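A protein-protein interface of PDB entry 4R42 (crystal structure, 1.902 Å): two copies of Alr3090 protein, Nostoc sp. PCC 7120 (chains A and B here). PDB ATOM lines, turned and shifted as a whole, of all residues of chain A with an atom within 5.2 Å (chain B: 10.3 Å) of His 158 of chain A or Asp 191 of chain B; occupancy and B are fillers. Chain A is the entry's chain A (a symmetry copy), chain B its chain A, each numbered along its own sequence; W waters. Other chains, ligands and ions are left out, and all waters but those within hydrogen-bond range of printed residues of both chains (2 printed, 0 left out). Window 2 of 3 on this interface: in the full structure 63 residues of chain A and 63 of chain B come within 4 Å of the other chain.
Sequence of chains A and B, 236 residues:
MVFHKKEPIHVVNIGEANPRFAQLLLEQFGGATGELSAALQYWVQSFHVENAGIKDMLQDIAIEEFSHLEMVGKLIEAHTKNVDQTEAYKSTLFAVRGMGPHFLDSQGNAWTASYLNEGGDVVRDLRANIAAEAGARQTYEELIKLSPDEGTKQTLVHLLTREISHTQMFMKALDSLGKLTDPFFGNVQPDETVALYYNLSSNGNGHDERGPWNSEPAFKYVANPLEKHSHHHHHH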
ATOM      1  N   ILE A   9      21.530 -10.789  10.037  1.00  0.00           N
ATOM      2  CA  ILE A   9      21.332 -12.225  10.209  1.00  0.00           C
ATOM      3  C   ILE A   9      19.849 -12.551  10.417  1.00  0.00           C
ATOM      4  O   ILE A   9      19.419 -13.674  10.153  1.00  0.00           O
ATOM      5  CB  ILE A   9      22.201 -12.794  11.378  1.00  0.00           C
ATOM      6  CG1 ILE A   9      23.220 -13.804  10.811  1.00  0.00           C
ATOM      7  CG2 ILE A   9      21.332 -13.392  12.510  1.00  0.00           C
ATOM      8  CD1 ILE A   9      23.485 -15.014  11.660  1.00  0.00           C
ATOM      9  N   HIS A  10      19.071 -11.576  10.880  1.00  0.00           N
ATOM     10  CA  HIS A  10      17.614 -11.661  10.763  1.00  0.00           C
ATOM     11  C   HIS A  10      16.979 -10.276  10.902  1.00  0.00           C
ATOM     12  O   HIS A  10      17.669  -9.289  11.166  1.00  0.00           O
ATOM     13  CB  HIS A  10      17.024 -12.658  11.780  1.00  0.00           C
ATOM     14  CG  HIS A  10      17.005 -12.180  13.201  1.00  0.00           C
ATOM     15  ND1 HIS A  10      16.402 -11.003  13.592  1.00  0.00           N
ATOM     16  CD2 HIS A  10      17.471 -12.756  14.335  1.00  0.00           C
ATOM     17  CE1 HIS A  10      16.523 -10.861  14.900  1.00  0.00           C
ATOM     18  NE2 HIS A  10      17.167 -11.911  15.375  1.00  0.00           N
ATOM     19  N   MET A  71      23.840  -6.671  14.083  1.00  0.00           N
ATOM     20  CA  MET A  71      22.472  -6.754  14.611  1.00  0.00           C
ATOM     21  C   MET A  71      22.275  -5.792  15.779  1.00  0.00           C
ATOM     22  O   MET A  71      21.246  -5.125  15.871  1.00  0.00           O
ATOM     23  CB  MET A  71      22.136  -8.178  15.078  1.00  0.00           C
ATOM     24  CG  MET A  71      22.044  -9.206  13.970  1.00  0.00           C
ATOM     25  SD  MET A  71      21.761 -10.889  14.598  1.00  0.00           S
ATOM     26  CE  MET A  71      20.411 -10.628  15.753  1.00  0.00           C
ATOM     27  N   LYS A 153      13.246  -7.849  22.593  1.00  0.00           N
ATOM     28  CA  LYS A 153      13.524  -8.963  23.490  1.00  0.00           C
ATOM     29  C   LYS A 153      13.878 -10.242  22.739  1.00  0.00           C
ATOM     30  O   LYS A 153      14.832 -10.918  23.089  1.00  0.00           O
ATOM     31  CB  LYS A 153      12.337  -9.239  24.406  1.00  0.00           C
ATOM     32  CG  LYS A 153      12.662 -10.332  25.420  1.00  0.00           C
ATOM     33  CD  LYS A 153      11.676 -10.403  26.560  1.00  0.00           C
ATOM     34  CE  LYS A 153      10.299 -10.821  26.095  1.00  0.00           C
ATOM     35  NZ  LYS A 153       9.438 -11.306  27.219  1.00  0.00           N
ATOM     36  N   GLN A 154      13.108 -10.579  21.711  1.00  0.00           N
ATOM     37  CA  GLN A 154      13.351 -11.813  20.985  1.00  0.00           C
ATOM     38  C   GLN A 154      14.710 -11.811  20.301  1.00  0.00           C
ATOM     39  O   GLN A 154      15.377 -12.847  20.232  1.00  0.00           O
ATOM     40  CB  GLN A 154      12.246 -12.064  19.949  1.00  0.00           C
ATOM     41  CG  GLN A 154      10.964 -12.630  20.546  1.00  0.00           C
ATOM     42  CD  GLN A 154      11.234 -13.752  21.551  1.00  0.00           C
ATOM     43  OE1 GLN A 154      11.629 -14.865  21.176  1.00  0.00           O
ATOM     44  NE2 GLN A 154      11.056 -13.449  22.838  1.00  0.00           N
ATOM     45  N   THR A 155      15.126 -10.657  19.802  1.00  0.00           N
ATOM     46  CA  THR A 155      16.460 -10.546  19.222  1.00  0.00           C
ATOM     47  C   THR A 155      17.553 -10.778  20.256  1.00  0.00           C
ATOM     48  O   THR A 155      18.530 -11.473  19.992  1.00  0.00           O
ATOM     49  CB  THR A 155      16.673  -9.173  18.582  1.00  0.00           C
ATOM     50  OG1 THR A 155      15.736  -9.011  17.524  1.00  0.00           O
ATOM     51  CG2 THR A 155      18.094  -9.040  18.025  1.00  0.00           C
ATOM     52  N   LEU A 156      17.396 -10.179  21.427  1.00  0.00           N
ATOM     53  CA  LEU A 156      18.346 -10.376  22.510  1.00  0.00           C
ATOM     54  C   LEU A 156      18.375 -11.831  22.981  1.00  0.00           C
ATOM     55  O   LEU A 156      19.438 -12.362  23.295  1.00  0.00           O
ATOM     56  CB  LEU A 156      18.013  -9.451  23.684  1.00  0.00           C
ATOM     57  CG  LEU A 156      18.065  -7.946  23.383  1.00  0.00           C
ATOM     58  CD1 LEU A 156      17.617  -7.153  24.594  1.00  0.00           C
ATOM     59  CD2 LEU A 156      19.440  -7.497  22.946  1.00  0.00           C
ATOM     60  N   VAL A 157      17.216 -12.480  23.032  1.00  0.00           N
ATOM     61  CA  VAL A 157      17.174 -13.877  23.439  1.00  0.00           C
ATOM     62  C   VAL A 157      17.952 -14.713  22.419  1.00  0.00           C
ATOM     63  O   VAL A 157      18.645 -15.664  22.786  1.00  0.00           O
ATOM     64  CB  VAL A 157      15.728 -14.384  23.588  1.00  0.00           C
ATOM     65  CG1 VAL A 157      15.675 -15.910  23.714  1.00  0.00           C
ATOM     66  CG2 VAL A 157      15.073 -13.754  24.815  1.00  0.00           C
ATOM     67  N   HIS A 158      17.837 -14.358  21.146  1.00  0.00           N
ATOM     68  CA  HIS A 158      18.553 -15.085  20.111  1.00  0.00           C
ATOM     69  C   HIS A 158      20.059 -14.924  20.280  1.00  0.00           C
ATOM     70  O   HIS A 158      20.801 -15.904  20.209  1.00  0.00           O
ATOM     71  CB  HIS A 158      18.148 -14.616  18.715  1.00  0.00           C
ATOM     72  CG  HIS A 158      18.990 -15.216  17.633  1.00  0.00           C
ATOM     73  ND1 HIS A 158      18.961 -16.560  17.331  1.00  0.00           N
ATOM     74  CD2 HIS A 158      19.923 -14.666  16.821  1.00  0.00           C
ATOM     75  CE1 HIS A 158      19.823 -16.809  16.361  1.00  0.00           C
ATOM     76  NE2 HIS A 158      20.419 -15.675  16.032  1.00  0.00           N
ATOM     77  N   LEU A 159      20.500 -13.689  20.492  1.00  0.00           N
ATOM     78  CA  LEU A 159      21.908 -13.409  20.684  1.00  0.00           C
ATOM     79  C   LEU A 159      22.422 -14.132  21.932  1.00  0.00           C
ATOM     80  O   LEU A 159      23.499 -14.717  21.911  1.00  0.00           O
ATOM     81  CB  LEU A 159      22.142 -11.907  20.783  1.00  0.00           C
ATOM     82  CG  LEU A 159      21.822 -11.139  19.493  1.00  0.00           C
ATOM     83  CD1 LEU A 159      21.737  -9.652  19.750  1.00  0.00           C
ATOM     84  CD2 LEU A 159      22.871 -11.461  18.416  1.00  0.00           C
ATOM     85  N   LEU A 160      21.647 -14.101  23.009  1.00  0.00           N
ATOM     86  CA  LEU A 160      22.021 -14.814  24.230  1.00  0.00           C
ATOM     87  C   LEU A 160      22.173 -16.308  23.940  1.00  0.00           C
ATOM     88  O   LEU A 160      23.114 -16.957  24.408  1.00  0.00           O
ATOM     89  CB  LEU A 160      20.974 -14.579  25.331  1.00  0.00           C
ATOM     90  CG  LEU A 160      21.209 -15.291  26.662  1.00  0.00           C
ATOM     91  CD1 LEU A 160      20.650 -14.489  27.841  1.00  0.00           C
ATOM     92  CD2 LEU A 160      20.589 -16.662  26.646  1.00  0.00           C
ATOM     93  N   THR A 161      21.237 -16.844  23.164  1.00  0.00           N
ATOM     94  CA  THR A 161      21.235 -18.267  22.838  1.00  0.00           C
ATOM     95  C   THR A 161      22.502 -18.637  22.067  1.00  0.00           C
ATOM     96  O   THR A 161      23.122 -19.675  22.331  1.00  0.00           O
ATOM     97  CB  THR A 161      19.997 -18.665  22.012  1.00  0.00           C
ATOM     98  OG1 THR A 161      18.800 -18.464  22.785  1.00  0.00           O
ATOM     99  CG2 THR A 161      20.077 -20.140  21.599  1.00  0.00           C
ATOM    100  N   ARG A 162      22.894 -17.788  21.122  1.00  0.00           N
ATOM    101  CA  ARG A 162      24.130 -18.022  20.374  1.00  0.00           C
ATOM    102  C   ARG A 162      25.393 -17.982  21.267  1.00  0.00           C
ATOM    103  O   ARG A 162      26.374 -18.661  20.961  1.00  0.00           O
ATOM    104  CB  ARG A 162      24.259 -17.008  19.231  1.00  0.00           C
ATOM    105  CG  ARG A 162      23.150 -17.119  18.158  1.00  0.00           C
ATOM    106  CD  ARG A 162      23.042 -18.546  17.579  1.00  0.00           C
ATOM    107  NE  ARG A 162      24.342 -18.971  17.070  1.00  0.00           N
ATOM    108  CZ  ARG A 162      24.738 -20.227  16.901  1.00  0.00           C
ATOM    109  NH1 ARG A 162      23.936 -21.245  17.196  1.00  0.00           N
ATOM    110  NH2 ARG A 162      25.955 -20.464  16.426  1.00  0.00           N
ATOM    111  N   PHE B 184      25.330 -24.048  29.705  1.00  0.00           N
ATOM    112  CA  PHE B 184      24.175 -23.238  30.045  1.00  0.00           C
ATOM    113  C   PHE B 184      24.225 -22.712  31.474  1.00  0.00           C
ATOM    114  O   PHE B 184      24.512 -23.452  32.410  1.00  0.00           O
ATOM    115  CB  PHE B 184      22.882 -24.036  29.846  1.00  0.00           C
ATOM    116  CG  PHE B 184      21.653 -23.250  30.190  1.00  0.00           C
ATOM    117  CD1 PHE B 184      21.134 -22.331  29.296  1.00  0.00           C
ATOM    118  CD2 PHE B 184      21.057 -23.380  31.428  1.00  0.00           C
ATOM    119  CE1 PHE B 184      20.032 -21.583  29.613  1.00  0.00           C
ATOM    120  CE2 PHE B 184      19.947 -22.631  31.759  1.00  0.00           C
ATOM    121  CZ  PHE B 184      19.429 -21.729  30.852  1.00  0.00           C
ATOM    122  N   VAL B 188      17.525 -17.338  31.495  1.00  0.00           N
ATOM    123  CA  VAL B 188      16.827 -17.133  30.234  1.00  0.00           C
ATOM    124  C   VAL B 188      16.759 -18.433  29.429  1.00  0.00           C
ATOM    125  O   VAL B 188      17.779 -19.040  29.109  1.00  0.00           O
ATOM    126  CB  VAL B 188      17.507 -16.045  29.390  1.00  0.00           C
ATOM    127  CG1 VAL B 188      16.734 -15.804  28.097  1.00  0.00           C
ATOM    128  CG2 VAL B 188      17.602 -14.760  30.185  1.00  0.00           C
ATOM    129  N   GLN B 189      15.542 -18.852  29.109  1.00  0.00           N
ATOM    130  CA  GLN B 189      15.336 -19.999  28.243  1.00  0.00           C
ATOM    131  C   GLN B 189      15.844 -19.695  26.828  1.00  0.00           C
ATOM    132  O   GLN B 189      15.440 -18.698  26.228  1.00  0.00           O
ATOM    133  CB  GLN B 189      13.856 -20.370  28.193  1.00  0.00           C
ATOM    134  CG  GLN B 189      13.572 -21.639  27.418  1.00  0.00           C
ATOM    135  CD  GLN B 189      12.093 -21.902  27.281  1.00  0.00           C
ATOM    136  OE1 GLN B 189      11.283 -21.422  28.079  1.00  0.00           O
ATOM    137  NE2 GLN B 189      11.724 -22.631  26.240  1.00  0.00           N
ATOM    138  N   PRO B 190      16.723 -20.550  26.286  1.00  0.00           N
ATOM    139  CA  PRO B 190      17.223 -20.324  24.920  1.00  0.00           C
ATOM    140  C   PRO B 190      16.141 -20.478  23.858  1.00  0.00           C
ATOM    141  O   PRO B 190      15.104 -21.087  24.143  1.00  0.00           O
ATOM    142  CB  PRO B 190      18.294 -21.408  24.754  1.00  0.00           C
ATOM    143  CG  PRO B 190      18.665 -21.798  26.151  1.00  0.00           C
ATOM    144  CD  PRO B 190      17.387 -21.705  26.916  1.00  0.00           C
ATOM    145  N   ASP B 191      16.371 -19.929  22.663  1.00  0.00           N
ATOM    146  CA  ASP B 191      15.470 -20.173  21.539  1.00  0.00           C
ATOM    147  C   ASP B 191      15.926 -21.448  20.813  1.00  0.00           C
ATOM    148  O   ASP B 191      16.719 -22.217  21.338  1.00  0.00           O
ATOM    149  CB  ASP B 191      15.386 -18.953  20.583  1.00  0.00           C
ATOM    150  CG  ASP B 191      16.651 -18.710  19.772  1.00  0.00           C
ATOM    151  OD1 ASP B 191      17.559 -19.563  19.730  1.00  0.00           O
ATOM    152  OD2 ASP B 191      16.729 -17.633  19.138  1.00  0.00           O
ATOM    153  N   GLU B 192      15.425 -21.662  19.605  1.00  0.00           N
ATOM    154  CA  GLU B 192      15.598 -22.944  18.930  1.00  0.00           C
ATOM    155  C   GLU B 192      16.935 -23.076  18.194  1.00  0.00           C
ATOM    156  O   GLU B 192      17.196 -24.094  17.563  1.00  0.00           O
ATOM    157  CB  GLU B 192      14.433 -23.177  17.949  1.00  0.00           C
ATOM    158  CG  GLU B 192      14.397 -22.252  16.726  1.00  0.00           C
ATOM    159  CD  GLU B 192      13.960 -20.825  17.047  1.00  0.00           C
ATOM    160  OE1 GLU B 192      13.572 -20.555  18.206  1.00  0.00           O
ATOM    161  OE2 GLU B 192      14.003 -19.969  16.133  1.00  0.00           O
ATOM    162  N   THR B 193      17.803 -22.075  18.295  1.00  0.00           N
ATOM    163  CA  THR B 193      19.024 -22.067  17.486  1.00  0.00           C
ATOM    164  C   THR B 193      20.295 -22.494  18.226  1.00  0.00           C
ATOM    165  O   THR B 193      21.397 -22.352  17.688  1.00  0.00           O
ATOM    166  CB  THR B 193      19.270 -20.659  16.886  1.00  0.00           C
ATOM    167  OG1 THR B 193      19.704 -19.764  17.912  1.00  0.00           O
ATOM    168  CG2 THR B 193      17.998 -20.118  16.245  1.00  0.00           C
ATOM    169  N   VAL B 194      20.163 -23.031  19.439  1.00  0.00           N
ATOM    170  CA  VAL B 194      21.338 -23.260  20.281  1.00  0.00           C
ATOM    171  C   VAL B 194      22.327 -24.286  19.699  1.00  0.00           C
ATOM    172  O   VAL B 194      23.523 -24.238  20.001  1.00  0.00           O
ATOM    173  CB  VAL B 194      20.934 -23.709  21.715  1.00  0.00           C
ATOM    174  CG1 VAL B 194      20.558 -25.197  21.765  1.00  0.00           C
ATOM    175  CG2 VAL B 194      22.061 -23.388  22.695  1.00  0.00           C
ATOM    176  N   ALA B 195      21.842 -25.187  18.844  1.00  0.00           N
ATOM    177  CA  ALA B 195      22.688 -26.266  18.327  1.00  0.00           C
ATOM    178  C   ALA B 195      23.319 -25.949  16.970  1.00  0.00           C
ATOM    179  O   ALA B 195      24.050 -26.766  16.419  1.00  0.00           O
ATOM    180  CB  ALA B 195      21.880 -27.557  18.237  1.00  0.00           C
ATOM    181  N   LEU B 196      23.049 -24.772  16.421  1.00  0.00           N
ATOM    182  CA  LEU B 196      23.527 -24.466  15.074  1.00  0.00           C
ATOM    183  C   LEU B 196      24.991 -24.039  15.075  1.00  0.00           C
ATOM    184  O   LEU B 196      25.423 -23.307  15.948  1.00  0.00           O
ATOM    185  CB  LEU B 196      22.679 -23.368  14.439  1.00  0.00           C
ATOM    186  CG  LEU B 196      21.204 -23.694  14.213  1.00  0.00           C
ATOM    187  CD1 LEU B 196      20.508 -22.462  13.667  1.00  0.00           C
ATOM    188  CD2 LEU B 196      21.057 -24.860  13.244  1.00  0.00           C
ATOM    189  N   TYR B 197      25.737 -24.498  14.073  1.00  0.00           N
ATOM    190  CA  TYR B 197      27.104 -24.023  13.840  1.00  0.00           C
ATOM    191  C   TYR B 197      27.213 -23.524  12.414  1.00  0.00           C
ATOM    192  O   TYR B 197      26.995 -24.285  11.472  1.00  0.00           O
ATOM    193  CB  TYR B 197      28.119 -25.137  14.084  1.00  0.00           C
ATOM    194  CG  TYR B 197      29.573 -24.721  13.930  1.00  0.00           C
ATOM    195  CD1 TYR B 197      30.153 -24.581  12.668  1.00  0.00           C
ATOM    196  CD2 TYR B 197      30.374 -24.491  15.049  1.00  0.00           C
ATOM    197  CE1 TYR B 197      31.483 -24.219  12.522  1.00  0.00           C
ATOM    198  CE2 TYR B 197      31.715 -24.126  14.914  1.00  0.00           C
ATOM    199  CZ  TYR B 197      32.263 -24.001  13.646  1.00  0.00           C
ATOM    200  OH  TYR B 197      33.588 -23.658  13.495  1.00  0.00           O
ATOM    201  N   TYR B 198      27.562 -22.251  12.262  1.00  0.00           N
ATOM    202  CA  TYR B 198      27.689 -21.647  10.947  1.00  0.00           C
ATOM    203  C   TYR B 198      29.127 -21.640  10.475  1.00  0.00           C
ATOM    204  O   TYR B 198      30.012 -21.089  11.133  1.00  0.00           O
ATOM    205  CB  TYR B 198      27.148 -20.221  10.964  1.00  0.00           C
ATOM    206  CG  TYR B 198      25.730 -20.120  11.457  1.00  0.00           C
ATOM    207  CD1 TYR B 198      24.670 -20.530  10.665  1.00  0.00           C
ATOM    208  CD2 TYR B 198      25.450 -19.598  12.715  1.00  0.00           C
ATOM    209  CE1 TYR B 198      23.363 -20.427  11.111  1.00  0.00           C
ATOM    210  CE2 TYR B 198      24.155 -19.493  13.172  1.00  0.00           C
ATOM    211  CZ  TYR B 198      23.116 -19.908  12.368  1.00  0.00           C
ATOM    212  OH  TYR B 198      21.822 -19.799  12.825  1.00  0.00           O
ATOM    213  N   LEU B 200      31.205 -19.925   8.688  1.00  0.00           N
ATOM    214  CA  LEU B 200      31.284 -18.592   8.108  1.00  0.00           C
ATOM    215  C   LEU B 200      32.674 -18.247   7.577  1.00  0.00           C
ATOM    216  O   LEU B 200      32.818 -17.297   6.809  1.00  0.00           O
ATOM    217  CB  LEU B 200      30.845 -17.564   9.142  1.00  0.00           C
ATOM    218  CG  LEU B 200      29.350 -17.605   9.464  1.00  0.00           C
ATOM    219  CD1 LEU B 200      29.071 -16.909  10.784  1.00  0.00           C
ATOM    220  CD2 LEU B 200      28.541 -16.974   8.333  1.00  0.00           C
HETATM  221  O   HOH W   1      14.516 -15.571  20.012  1.00  0.00           O
HETATM  222  O   HOH W   2      28.417 -20.716  14.619  1.00  0.00           O
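OD2 of Asp 191 of chain B lies within hydrogen-bond range of ND1 of His 158 of chain A.
A ring nitrogen (ND1) of His 158 of chain A lies close to the side-chain hydroxyl (OG1) of Thr 193 of chain B.
O of Leu 196 of chain B lies within hydrogen-bond range of NH1 of Arg 162 of chain A (2.8 Å).
The side-chain hydroxyl of Thr 161 of chain A sits at hydrogen-bond distance from the backbone NH of Asp 191 of chain B (2.8 Å).
The guanidinium group (NH1) of Arg 162 of chain A lies within hydrogen-bond range of the backbone carbonyl oxygen (O) of Thr 193 of chain B.
No position is printed for both chains.
Of the 11 pairs that touch across the chains among the printed residues, none has its exchanged pair printed and touching as well.
Water W1 bridges O of Gln 154 of chain A (2.9 Å) and OD2 of Asp 191 of chain B (3.1 Å).
Water W2 lies within hydrogen-bond range of the backbone NH of Tyr 198 of chain B (2.9 Å) and the guanidinium group of Arg 162 of chain A (3.1 Å).
His 158 of chain A touches just these residues of chain B: Asp 191 (3.1 Å) and Thr 193 (3.3 Å).
Of chain A, only His 158 (3.1 Å) and Thr 161 (2.8 Å) come within 4 Å of Asp 191 of chain B.
No residue of chain B comes within 4 Å of Thr 155 of chain A.
Val 157 of chain A touches just one residue of chain B: Gln 189.
No residue of chain B comes within 4 Å of Leu 159 of chain A.
Printed residues of chain A within 4 Å of Pro 190 of chain B: Thr 161.
Of the printed residues of chain A, Tyr 198 of chain B touches Arg 162 (3.8 Å).
Of the printed residues of chain B, Leu 160 of chain A touches Val 188.
Of the printed residues of chain A, Gln 189 of chain B touches Val 157.
Of the printed residues of chain A, Val 188 of chain B touches Leu 160.
Met 71 of chain A touches none of the printed residues of chain B.
The nearest residue of chain B that does not touch His 158 of chain A is Tyr 198 of chain B (5.0 Å).
The nearest residue of chain A that does not touch Asp 191 of chain B is Val 157 of chain A (4.2 Å).
The nearest printed residue of chain A that does not touch Pro 190 of chain B is Val 157 of chain A (4.6 Å).
The backbone carbonyl oxygen (O) of Val 157 of chain A lies within hydrogen-bond range of the side-chain hydroxyl (OG1) of Thr 161 of chain A, at 2.8 Å.
The side-chain carboxylate (OD1) of Asp 191 of chain B is in hydrogen-bond range of the side-chain hydroxyl (OG1) of Thr 193 of chain B.
Of the 13 printed residues of chain B, 8 touch a printed residue of chain A.
Printed residues of chain B that touch a printed residue of chain A: Val 188, Gln 189, Pro 190, Asp 191, Thr 193, Val 194, Leu 196 and Tyr 198.
Hydrophobic or aromatic side chains of chain B within 4 Å of the printed part of chain A: Val 188, Pro 190, Val 194, Leu 196 and Tyr 198.
Among the printed residues, 11 pairs touch across the chains.
Among the printed residues, no Asp or Glu carboxylate lies within 4 Å of a Lys or Arg side-chain nitrogen of the other chain.
Gln 189 of chain B touches Val 157 of chain A (O to CG1, 3.8 Å).
Leu 160 of chain A touches Val 188 of chain B.
Thr 161 of chain A touches Pro 190 of chain B.
OG1 of Thr 193 of chain B touches CG2 of Thr 161 of chain A, 3.7 Å away.
CG2 of Thr 161 of chain A touches N of Val 194 of chain B, 3.6 Å away.
Arg 162 of chain A touches Tyr 198 of chain B.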
